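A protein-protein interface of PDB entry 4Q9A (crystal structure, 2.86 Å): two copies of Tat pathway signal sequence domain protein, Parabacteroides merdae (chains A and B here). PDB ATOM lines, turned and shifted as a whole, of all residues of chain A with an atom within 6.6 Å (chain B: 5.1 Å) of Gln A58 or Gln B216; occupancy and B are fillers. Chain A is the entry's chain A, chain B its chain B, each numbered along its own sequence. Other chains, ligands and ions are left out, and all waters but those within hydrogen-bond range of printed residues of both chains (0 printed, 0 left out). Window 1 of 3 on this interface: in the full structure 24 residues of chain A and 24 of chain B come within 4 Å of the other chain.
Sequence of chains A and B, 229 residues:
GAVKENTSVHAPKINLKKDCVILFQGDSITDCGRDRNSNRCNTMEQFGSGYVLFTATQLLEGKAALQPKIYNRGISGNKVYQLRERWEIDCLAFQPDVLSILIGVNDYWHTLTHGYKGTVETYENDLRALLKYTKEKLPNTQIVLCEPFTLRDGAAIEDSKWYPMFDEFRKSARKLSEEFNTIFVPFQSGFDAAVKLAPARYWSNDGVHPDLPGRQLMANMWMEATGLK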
ATOM      1  N   LEU A  53       3.726   4.499   3.573  1.00  0.00           N
ATOM      2  CA  LEU A  53       5.126   4.897   3.512  1.00  0.00           C
ATOM      3  C   LEU A  53       5.297   6.339   4.058  1.00  0.00           C
ATOM      4  O   LEU A  53       6.104   6.564   4.958  1.00  0.00           O
ATOM      5  CB  LEU A  53       5.642   4.768   2.057  1.00  0.00           C
ATOM      6  CG  LEU A  53       6.892   5.553   1.645  1.00  0.00           C
ATOM      7  CD1 LEU A  53       8.125   5.070   2.399  1.00  0.00           C
ATOM      8  CD2 LEU A  53       7.119   5.454   0.151  1.00  0.00           C
ATOM      9  N   PHE A  54       4.484   7.281   3.551  1.00  0.00           N
ATOM     10  CA  PHE A  54       4.541   8.699   3.881  1.00  0.00           C
ATOM     11  C   PHE A  54       4.124   9.003   5.317  1.00  0.00           C
ATOM     12  O   PHE A  54       4.646   9.956   5.893  1.00  0.00           O
ATOM     13  CB  PHE A  54       3.731   9.496   2.866  1.00  0.00           C
ATOM     14  CG  PHE A  54       4.361   9.350   1.500  1.00  0.00           C
ATOM     15  CD1 PHE A  54       5.563   9.991   1.197  1.00  0.00           C
ATOM     16  CD2 PHE A  54       3.809   8.496   0.551  1.00  0.00           C
ATOM     17  CE1 PHE A  54       6.189   9.801  -0.044  1.00  0.00           C
ATOM     18  CE2 PHE A  54       4.420   8.317  -0.695  1.00  0.00           C
ATOM     19  CZ  PHE A  54       5.607   8.975  -0.986  1.00  0.00           C
ATOM     20  N   THR A  55       3.243   8.182   5.895  1.00  0.00           N
ATOM     21  CA  THR A  55       2.789   8.288   7.281  1.00  0.00           C
ATOM     22  C   THR A  55       3.885   7.738   8.196  1.00  0.00           C
ATOM     23  O   THR A  55       4.211   8.345   9.216  1.00  0.00           O
ATOM     24  CB  THR A  55       1.475   7.503   7.467  1.00  0.00           C
ATOM     25  OG1 THR A  55       0.633   7.687   6.329  1.00  0.00           O
ATOM     26  CG2 THR A  55       0.738   7.882   8.737  1.00  0.00           C
ATOM     27  N   ALA A  56       4.439   6.565   7.821  1.00  0.00           N
ATOM     28  CA  ALA A  56       5.480   5.861   8.557  1.00  0.00           C
ATOM     29  C   ALA A  56       6.718   6.736   8.747  1.00  0.00           C
ATOM     30  O   ALA A  56       7.180   6.905   9.880  1.00  0.00           O
ATOM     31  CB  ALA A  56       5.841   4.582   7.840  1.00  0.00           C
ATOM     32  N   THR A  57       7.208   7.348   7.652  1.00  0.00           N
ATOM     33  CA  THR A  57       8.408   8.184   7.657  1.00  0.00           C
ATOM     34  C   THR A  57       8.218   9.419   8.575  1.00  0.00           C
ATOM     35  O   THR A  57       9.165   9.796   9.280  1.00  0.00           O
ATOM     36  CB  THR A  57       8.799   8.545   6.246  1.00  0.00           C
ATOM     37  OG1 THR A  57       7.667   9.096   5.569  1.00  0.00           O
ATOM     38  CG2 THR A  57       9.350   7.346   5.481  1.00  0.00           C
ATOM     39  N   GLN A  58       6.983   9.979   8.633  1.00  0.00           N
ATOM     40  CA  GLN A  58       6.653  11.100   9.521  1.00  0.00           C
ATOM     41  C   GLN A  58       6.725  10.644  10.968  1.00  0.00           C
ATOM     42  O   GLN A  58       7.208  11.390  11.828  1.00  0.00           O
ATOM     43  CB  GLN A  58       5.260  11.667   9.207  1.00  0.00           C
ATOM     44  CG  GLN A  58       5.217  12.440   7.910  1.00  0.00           C
ATOM     45  CD  GLN A  58       3.955  13.236   7.787  1.00  0.00           C
ATOM     46  OE1 GLN A  58       3.642  14.071   8.638  1.00  0.00           O
ATOM     47  NE2 GLN A  58       3.238  13.050   6.685  1.00  0.00           N
ATOM     48  N   LEU A  59       6.279   9.387  11.221  1.00  0.00           N
ATOM     49  CA  LEU A  59       6.301   8.763  12.537  1.00  0.00           C
ATOM     50  C   LEU A  59       7.751   8.424  12.943  1.00  0.00           C
ATOM     51  O   LEU A  59       8.171   8.731  14.068  1.00  0.00           O
ATOM     52  CB  LEU A  59       5.418   7.503  12.525  1.00  0.00           C
ATOM     53  CG  LEU A  59       3.908   7.729  12.593  1.00  0.00           C
ATOM     54  CD1 LEU A  59       3.130   6.497  12.119  1.00  0.00           C
ATOM     55  CD2 LEU A  59       3.485   8.165  13.982  1.00  0.00           C
ATOM     56  N   LEU A  60       8.519   7.842  12.005  1.00  0.00           N
ATOM     57  CA  LEU A  60       9.926   7.473  12.197  1.00  0.00           C
ATOM     58  C   LEU A  60      10.824   8.696  12.457  1.00  0.00           C
ATOM     59  O   LEU A  60      11.773   8.588  13.221  1.00  0.00           O
ATOM     60  CB  LEU A  60      10.468   6.706  10.961  1.00  0.00           C
ATOM     61  CG  LEU A  60       9.948   5.295  10.703  1.00  0.00           C
ATOM     62  CD1 LEU A  60      10.487   4.754   9.400  1.00  0.00           C
ATOM     63  CD2 LEU A  60      10.318   4.366  11.822  1.00  0.00           C
ATOM     64  N   GLU A  61      10.551   9.836  11.798  1.00  0.00           N
ATOM     65  CA  GLU A  61      11.348  11.055  11.984  1.00  0.00           C
ATOM     66  C   GLU A  61      10.838  11.842  13.230  1.00  0.00           C
ATOM     67  O   GLU A  61      11.625  12.189  14.121  1.00  0.00           O
ATOM     68  CB  GLU A  61      11.295  11.931  10.697  1.00  0.00           C
ATOM     69  CG  GLU A  61      12.077  13.234  10.759  1.00  0.00           C
ATOM     70  CD  GLU A  61      11.389  14.411  11.425  1.00  0.00           C
ATOM     71  OE1 GLU A  61      10.137  14.488  11.359  1.00  0.00           O
ATOM     72  OE2 GLU A  61      12.106  15.270  11.995  1.00  0.00           O
ATOM     73  N   GLY A  62       9.533  12.122  13.237  1.00  0.00           N
ATOM     74  CA  GLY A  62       8.866  12.870  14.282  1.00  0.00           C
ATOM     75  C   GLY A  62       8.974  12.280  15.665  1.00  0.00           C
ATOM     76  O   GLY A  62       9.356  12.993  16.598  1.00  0.00           O
ATOM     77  N   LYS A  63       8.643  10.969  15.800  1.00  0.00           N
ATOM     78  CA  LYS A  63       8.654  10.271  17.083  1.00  0.00           C
ATOM     79  C   LYS A  63       9.874   9.331  17.187  1.00  0.00           C
ATOM     80  O   LYS A  63       9.791   8.243  17.773  1.00  0.00           O
ATOM     81  CB  LYS A  63       7.326   9.502  17.247  1.00  0.00           C
ATOM     82  CG  LYS A  63       6.043  10.330  17.060  1.00  0.00           C
ATOM     83  CD  LYS A  63       5.793  11.402  18.137  1.00  0.00           C
ATOM     84  CE  LYS A  63       4.510  12.161  17.858  1.00  0.00           C
ATOM     85  NZ  LYS A  63       4.461  13.474  18.555  1.00  0.00           N
ATOM     86  N   ALA A  64      11.024   9.770  16.632  1.00  0.00           N
ATOM     87  CA  ALA A  64      12.301   9.031  16.580  1.00  0.00           C
ATOM     88  C   ALA A  64      12.820   8.562  17.952  1.00  0.00           C
ATOM     89  O   ALA A  64      13.354   7.456  18.047  1.00  0.00           O
ATOM     90  CB  ALA A  64      13.357   9.885  15.921  1.00  0.00           C
ATOM     91  N   GLN A 216       0.599  11.763   0.195  1.00  0.00           N
ATOM     92  CA  GLN A 216       1.142  12.751   1.120  1.00  0.00           C
ATOM     93  C   GLN A 216       0.000  13.411   1.899  1.00  0.00           C
ATOM     94  O   GLN A 216       0.103  13.503   3.120  1.00  0.00           O
ATOM     95  CB  GLN A 216       1.994  13.799   0.367  1.00  0.00           C
ATOM     96  CG  GLN A 216       2.822  14.724   1.271  1.00  0.00           C
ATOM     97  CD  GLN A 216       3.851  14.006   2.136  1.00  0.00           C
ATOM     98  OE1 GLN A 216       5.006  13.767   1.722  1.00  0.00           O
ATOM     99  NE2 GLN A 216       3.470  13.706   3.383  1.00  0.00           N
ATOM    100  N   ALA A 219      -1.411  10.969   4.503  1.00  0.00           N
ATOM    101  CA  ALA A 219      -0.402  10.855   5.561  1.00  0.00           C
ATOM    102  C   ALA A 219      -0.538  12.013   6.556  1.00  0.00           C
ATOM    103  O   ALA A 219      -0.587  11.778   7.764  1.00  0.00           O
ATOM    104  CB  ALA A 219       1.000  10.839   4.959  1.00  0.00           C
ATOM    105  N   ASN A 220      -0.668  13.249   6.039  1.00  0.00           N
ATOM    106  CA  ASN A 220      -0.812  14.467   6.831  1.00  0.00           C
ATOM    107  C   ASN A 220      -2.106  14.446   7.650  1.00  0.00           C
ATOM    108  O   ASN A 220      -2.098  14.862   8.814  1.00  0.00           O
ATOM    109  CB  ASN A 220      -0.778  15.699   5.922  1.00  0.00           C
ATOM    110  CG  ASN A 220       0.519  15.936   5.177  1.00  0.00           C
ATOM    111  OD1 ASN A 220       1.556  15.310   5.439  1.00  0.00           O
ATOM    112  ND2 ASN A 220       0.494  16.881   4.244  1.00  0.00           N
ATOM    113  N   MET A 221      -3.204  13.941   7.048  1.00  0.00           N
ATOM    114  CA  MET A 221      -4.513  13.823   7.701  1.00  0.00           C
ATOM    115  C   MET A 221      -4.439  12.867   8.897  1.00  0.00           C
ATOM    116  O   MET A 221      -4.913  13.180   9.993  1.00  0.00           O
ATOM    117  CB  MET A 221      -5.557  13.327   6.706  1.00  0.00           C
ATOM    118  CG  MET A 221      -5.900  14.339   5.632  1.00  0.00           C
ATOM    119  SD  MET A 221      -7.677  14.015   4.923  1.00  0.00           S
ATOM    120  CE  MET A 221      -8.681  14.554   6.506  1.00  0.00           C
ATOM    121  N   MET A 223      -1.648  11.901  10.505  1.00  0.00           N
ATOM    122  CA  MET A 223      -0.818  12.446  11.580  1.00  0.00           C
ATOM    123  C   MET A 223      -1.621  13.459  12.407  1.00  0.00           C
ATOM    124  O   MET A 223      -1.523  13.458  13.627  1.00  0.00           O
ATOM    125  CB  MET A 223       0.456  13.073  11.020  1.00  0.00           C
ATOM    126  CG  MET A 223       1.408  12.059  10.418  1.00  0.00           C
ATOM    127  SD  MET A 223       2.048  10.743  11.688  1.00  0.00           S
ATOM    128  CE  MET A 223       3.409  11.847  12.517  1.00  0.00           C
ATOM    129  N   LEU A 228      -0.480  13.134  16.406  1.00  0.00           N
ATOM    130  CA  LEU A 228       0.952  12.838  16.466  1.00  0.00           C
ATOM    131  C   LEU A 228       1.811  13.889  15.669  1.00  0.00           C
ATOM    132  O   LEU A 228       2.873  13.539  15.128  1.00  0.00           O
ATOM    133  CB  LEU A 228       1.215  11.395  15.981  1.00  0.00           C
ATOM    134  CG  LEU A 228       0.516  10.276  16.764  1.00  0.00           C
ATOM    135  CD1 LEU A 228       0.439   8.997  15.950  1.00  0.00           C
ATOM    136  CD2 LEU A 228       1.188  10.019  18.085  1.00  0.00           C
ATOM    137  N   LYS A 229       1.360  15.184  15.681  1.00  0.00           N
ATOM    138  CA  LYS A 229       1.922  16.413  15.080  1.00  0.00           C
ATOM    139  C   LYS A 229       1.428  16.586  13.638  1.00  0.00           C
ATOM    140  O   LYS A 229       1.602  15.647  12.842  1.00  0.00           O
ATOM    141  CB  LYS A 229       3.468  16.498  15.146  1.00  0.00           C
ATOM    142  OXT LYS A 229       0.832  17.640  13.317  1.00  0.00           O
ATOM    143  N   PHE B  54      10.511  12.446  -0.774  1.00  0.00           N
ATOM    144  CA  PHE B  54       9.822  13.005   0.381  1.00  0.00           C
ATOM    145  C   PHE B  54       9.665  14.529   0.306  1.00  0.00           C
ATOM    146  O   PHE B  54       8.682  15.058   0.820  1.00  0.00           O
ATOM    147  CB  PHE B  54      10.524  12.552   1.670  1.00  0.00           C
ATOM    148  CG  PHE B  54      10.420  11.047   1.790  1.00  0.00           C
ATOM    149  CD1 PHE B  54       9.205  10.438   2.114  1.00  0.00           C
ATOM    150  CD2 PHE B  54      11.503  10.232   1.481  1.00  0.00           C
ATOM    151  CE1 PHE B  54       9.090   9.048   2.166  1.00  0.00           C
ATOM    152  CE2 PHE B  54      11.389   8.840   1.534  1.00  0.00           C
ATOM    153  CZ  PHE B  54      10.187   8.255   1.885  1.00  0.00           C
ATOM    154  N   GLN B  58       5.870  16.645  -0.730  1.00  0.00           N
ATOM    155  CA  GLN B  58       5.481  17.803   0.095  1.00  0.00           C
ATOM    156  C   GLN B  58       5.203  18.994  -0.801  1.00  0.00           C
ATOM    157  O   GLN B  58       4.260  19.745  -0.547  1.00  0.00           O
ATOM    158  CB  GLN B  58       6.564  18.145   1.121  1.00  0.00           C
ATOM    159  CG  GLN B  58       6.662  17.125   2.247  1.00  0.00           C
ATOM    160  CD  GLN B  58       7.475  17.632   3.392  1.00  0.00           C
ATOM    161  OE1 GLN B  58       7.167  18.677   3.980  1.00  0.00           O
ATOM    162  NE2 GLN B  58       8.480  16.858   3.791  1.00  0.00           N
ATOM    163  N   LEU B 212      15.324   5.851   5.716  1.00  0.00           N
ATOM    164  CA  LEU B 212      13.986   6.459   5.766  1.00  0.00           C
ATOM    165  C   LEU B 212      13.808   7.587   6.827  1.00  0.00           C
ATOM    166  O   LEU B 212      13.341   8.663   6.423  1.00  0.00           O
ATOM    167  CB  LEU B 212      12.896   5.403   5.918  1.00  0.00           C
ATOM    168  CG  LEU B 212      12.776   4.416   4.730  1.00  0.00           C
ATOM    169  CD1 LEU B 212      11.749   3.362   5.010  1.00  0.00           C
ATOM    170  CD2 LEU B 212      12.444   5.132   3.417  1.00  0.00           C
ATOM    171  N   PRO B 213      14.238   7.453   8.123  1.00  0.00           N
ATOM    172  CA  PRO B 213      14.068   8.588   9.064  1.00  0.00           C
ATOM    173  C   PRO B 213      14.904   9.817   8.701  1.00  0.00           C
ATOM    174  O   PRO B 213      14.482  10.943   8.958  1.00  0.00           O
ATOM    175  CB  PRO B 213      14.521   8.009  10.398  1.00  0.00           C
ATOM    176  CG  PRO B 213      14.471   6.524  10.217  1.00  0.00           C
ATOM    177  CD  PRO B 213      14.857   6.300   8.810  1.00  0.00           C
ATOM    178  N   GLY B 214      16.063   9.592   8.095  1.00  0.00           N
ATOM    179  CA  GLY B 214      16.962  10.659   7.689  1.00  0.00           C
ATOM    180  C   GLY B 214      16.498  11.393   6.451  1.00  0.00           C
ATOM    181  O   GLY B 214      16.740  12.600   6.326  1.00  0.00           O
ATOM    182  N   ARG B 215      15.815  10.675   5.520  1.00  0.00           N
ATOM    183  CA  ARG B 215      15.305  11.257   4.261  1.00  0.00           C
ATOM    184  C   ARG B 215      14.160  12.221   4.561  1.00  0.00           C
ATOM    185  O   ARG B 215      14.137  13.339   4.030  1.00  0.00           O
ATOM    186  CB  ARG B 215      14.845  10.153   3.296  1.00  0.00           C
ATOM    187  CG  ARG B 215      15.978   9.273   2.796  1.00  0.00           C
ATOM    188  CD  ARG B 215      15.466   7.956   2.310  1.00  0.00           C
ATOM    189  NE  ARG B 215      16.572   7.016   2.159  1.00  0.00           N
ATOM    190  CZ  ARG B 215      16.462   5.790   1.655  1.00  0.00           C
ATOM    191  NH1 ARG B 215      15.281   5.335   1.241  1.00  0.00           N
ATOM    192  NH2 ARG B 215      17.530   5.006   1.562  1.00  0.00           N
ATOM    193  N   GLN B 216      13.226  11.786   5.448  1.00  0.00           N
ATOM    194  CA  GLN B 216      12.101  12.593   5.899  1.00  0.00           C
ATOM    195  C   GLN B 216      12.623  13.861   6.579  1.00  0.00           C
ATOM    196  O   GLN B 216      12.131  14.946   6.269  1.00  0.00           O
ATOM    197  CB  GLN B 216      11.172  11.789   6.823  1.00  0.00           C
ATOM    198  CG  GLN B 216       9.835  12.474   7.128  1.00  0.00           C
ATOM    199  CD  GLN B 216       8.946  12.713   5.926  1.00  0.00           C
ATOM    200  OE1 GLN B 216       8.153  11.846   5.529  1.00  0.00           O
ATOM    201  NE2 GLN B 216       9.012  13.916   5.356  1.00  0.00           N
ATOM    202  N   LEU B 217      13.662  13.734   7.438  1.00  0.00           N
ATOM    203  CA  LEU B 217      14.294  14.852   8.163  1.00  0.00           C
ATOM    204  C   LEU B 217      14.827  15.914   7.214  1.00  0.00           C
ATOM    205  O   LEU B 217      14.570  17.115   7.419  1.00  0.00           O
ATOM    206  CB  LEU B 217      15.443  14.331   9.034  1.00  0.00           C
ATOM    207  CG  LEU B 217      16.127  15.346   9.932  1.00  0.00           C
ATOM    208  CD1 LEU B 217      15.307  15.610  11.172  1.00  0.00           C
ATOM    209  CD2 LEU B 217      17.471  14.845  10.370  1.00  0.00           C
ATOM    210  N   MET B 218      15.596  15.460   6.183  1.00  0.00           N
ATOM    211  CA  MET B 218      16.181  16.289   5.122  1.00  0.00           C
ATOM    212  C   MET B 218      15.088  16.986   4.321  1.00  0.00           C
ATOM    213  O   MET B 218      15.198  18.190   4.096  1.00  0.00           O
ATOM    214  CB  MET B 218      17.035  15.443   4.204  1.00  0.00           C
ATOM    215  CG  MET B 218      18.314  14.981   4.854  1.00  0.00           C
ATOM    216  SD  MET B 218      19.226  13.690   3.738  1.00  0.00           S
ATOM    217  CE  MET B 218      19.794  14.794   2.405  1.00  0.00           C
ATOM    218  N   ALA B 219      14.001  16.266   3.956  1.00  0.00           N
ATOM    219  CA  ALA B 219      12.855  16.819   3.221  1.00  0.00           C
ATOM    220  C   ALA B 219      12.237  17.993   3.986  1.00  0.00           C
ATOM    221  O   ALA B 219      12.014  19.056   3.403  1.00  0.00           O
ATOM    222  CB  ALA B 219      11.811  15.739   2.986  1.00  0.00           C
ATOM    223  N   ASN B 220      12.022  17.816   5.300  1.00  0.00           N
ATOM    224  CA  ASN B 220      11.439  18.830   6.188  1.00  0.00           C
ATOM    225  C   ASN B 220      12.336  20.071   6.280  1.00  0.00           C
ATOM    226  O   ASN B 220      11.829  21.196   6.270  1.00  0.00           O
ATOM    227  CB  ASN B 220      11.215  18.233   7.591  1.00  0.00           C
ATOM    228  CG  ASN B 220      10.221  17.103   7.667  1.00  0.00           C
ATOM    229  OD1 ASN B 220       9.467  16.817   6.724  1.00  0.00           O
ATOM    230  ND2 ASN B 220      10.169  16.474   8.826  1.00  0.00           N
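Of the printed residues of chain B, Phe A54 touches Phe B54 (3.7 Å). Of the printed residues of chain B, Thr A57 touches Phe B54 (3.7 Å) and Gln B216 (2.8 Å). Gln A58 touches just one residue of chain B: Gln B216. Of the printed residues of chain A, Gln B216 touches Thr A57 (2.8 Å), Gln A58 (3.8 Å) and Glu A61 (3.9 Å). Printed residues of chain A within 4 Å of Asn B220: Glu A61 (3.2 Å). The nearest printed residue of chain B that does not touch Gln A58 is Asn B220 (6.2 Å). The nearest printed residue of chain A that does not touch Gln B216 is Phe A54 (4.0005 Å). The nearest printed residue of chain B that does not touch Gln A216 is Gln B216 (5.3 Å).
CD1 of Leu A53 touches CZ of Phe B54, at 3.8 Å. CE1 of Phe B54 touches CE1 of Phe A54 (3.7 Å). Thr A57 touches Phe B54. Gln A58 touches Gln B216 (N to OE1, 3.8 Å). O of Leu A60 touches CB of Pro B213, 3.98 Å away. Glu A61 touches Pro B213 (CB to O, 3.8 Å). Glu A61 touches Gln B216 (CB to CB, 3.9 Å). Leu B217 touches Glu A61 (CD1 to OE2, 3.3 Å). OE1 of Gln A216 touches O of Phe B54, at 3.999 Å. Gln B58 touches Gln A216.
The side-chain hydroxyl (OG1) of Thr A57 sits at hydrogen-bond distance from the side-chain amide oxygen (OE1) of Gln B216 (2.8 Å). The side-chain carboxylate (OE1) of Glu A61 sits at hydrogen-bond distance from the side-chain amide nitrogen (ND2) of Asn B220, at 3.2 Å.
Phe B54 touches its own counterpart, Phe A54. Gln A58 touches Gln B216, and with the chains exchanged Gln A216 touches Gln B58. Gln A216 touches Phe B54, but with the chains exchanged Phe A54 does not touch Gln B216 (4.0005 Å). Positions printed for both chains: 54, 58, 216, 219 and 220.
The side-chain amide nitrogen of Gln B216 lies close to the side-chain amide nitrogen of Gln B58. The backbone carbonyl oxygen (O) of Phe A54 sits close to the side-chain amide nitrogen (NE2) of Gln A58 (3.5 Å). OD1 of Asn A220 is in hydrogen-bond range of NE2 of Gln A58. The backbone carbonyl oxygen (O) of Phe B54 sits close to the side-chain amide nitrogen (NE2) of Gln B58, at 3.5 Å. NE2 of Gln A216 sits at hydrogen-bond distance from OD1 of Asn A220 (3.2 Å). OD1 of Asn B220 sits at hydrogen-bond distance from NE2 of Gln B58 (3.1 Å).
Hydrophobic or aromatic side chains of chain B that line the printed part of chain A: Phe B54, Pro B213 and Leu B217. Among the printed residues, no Asp or Glu carboxylate lies within 4 Å of a Lys or Arg side-chain nitrogen of the other chain.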
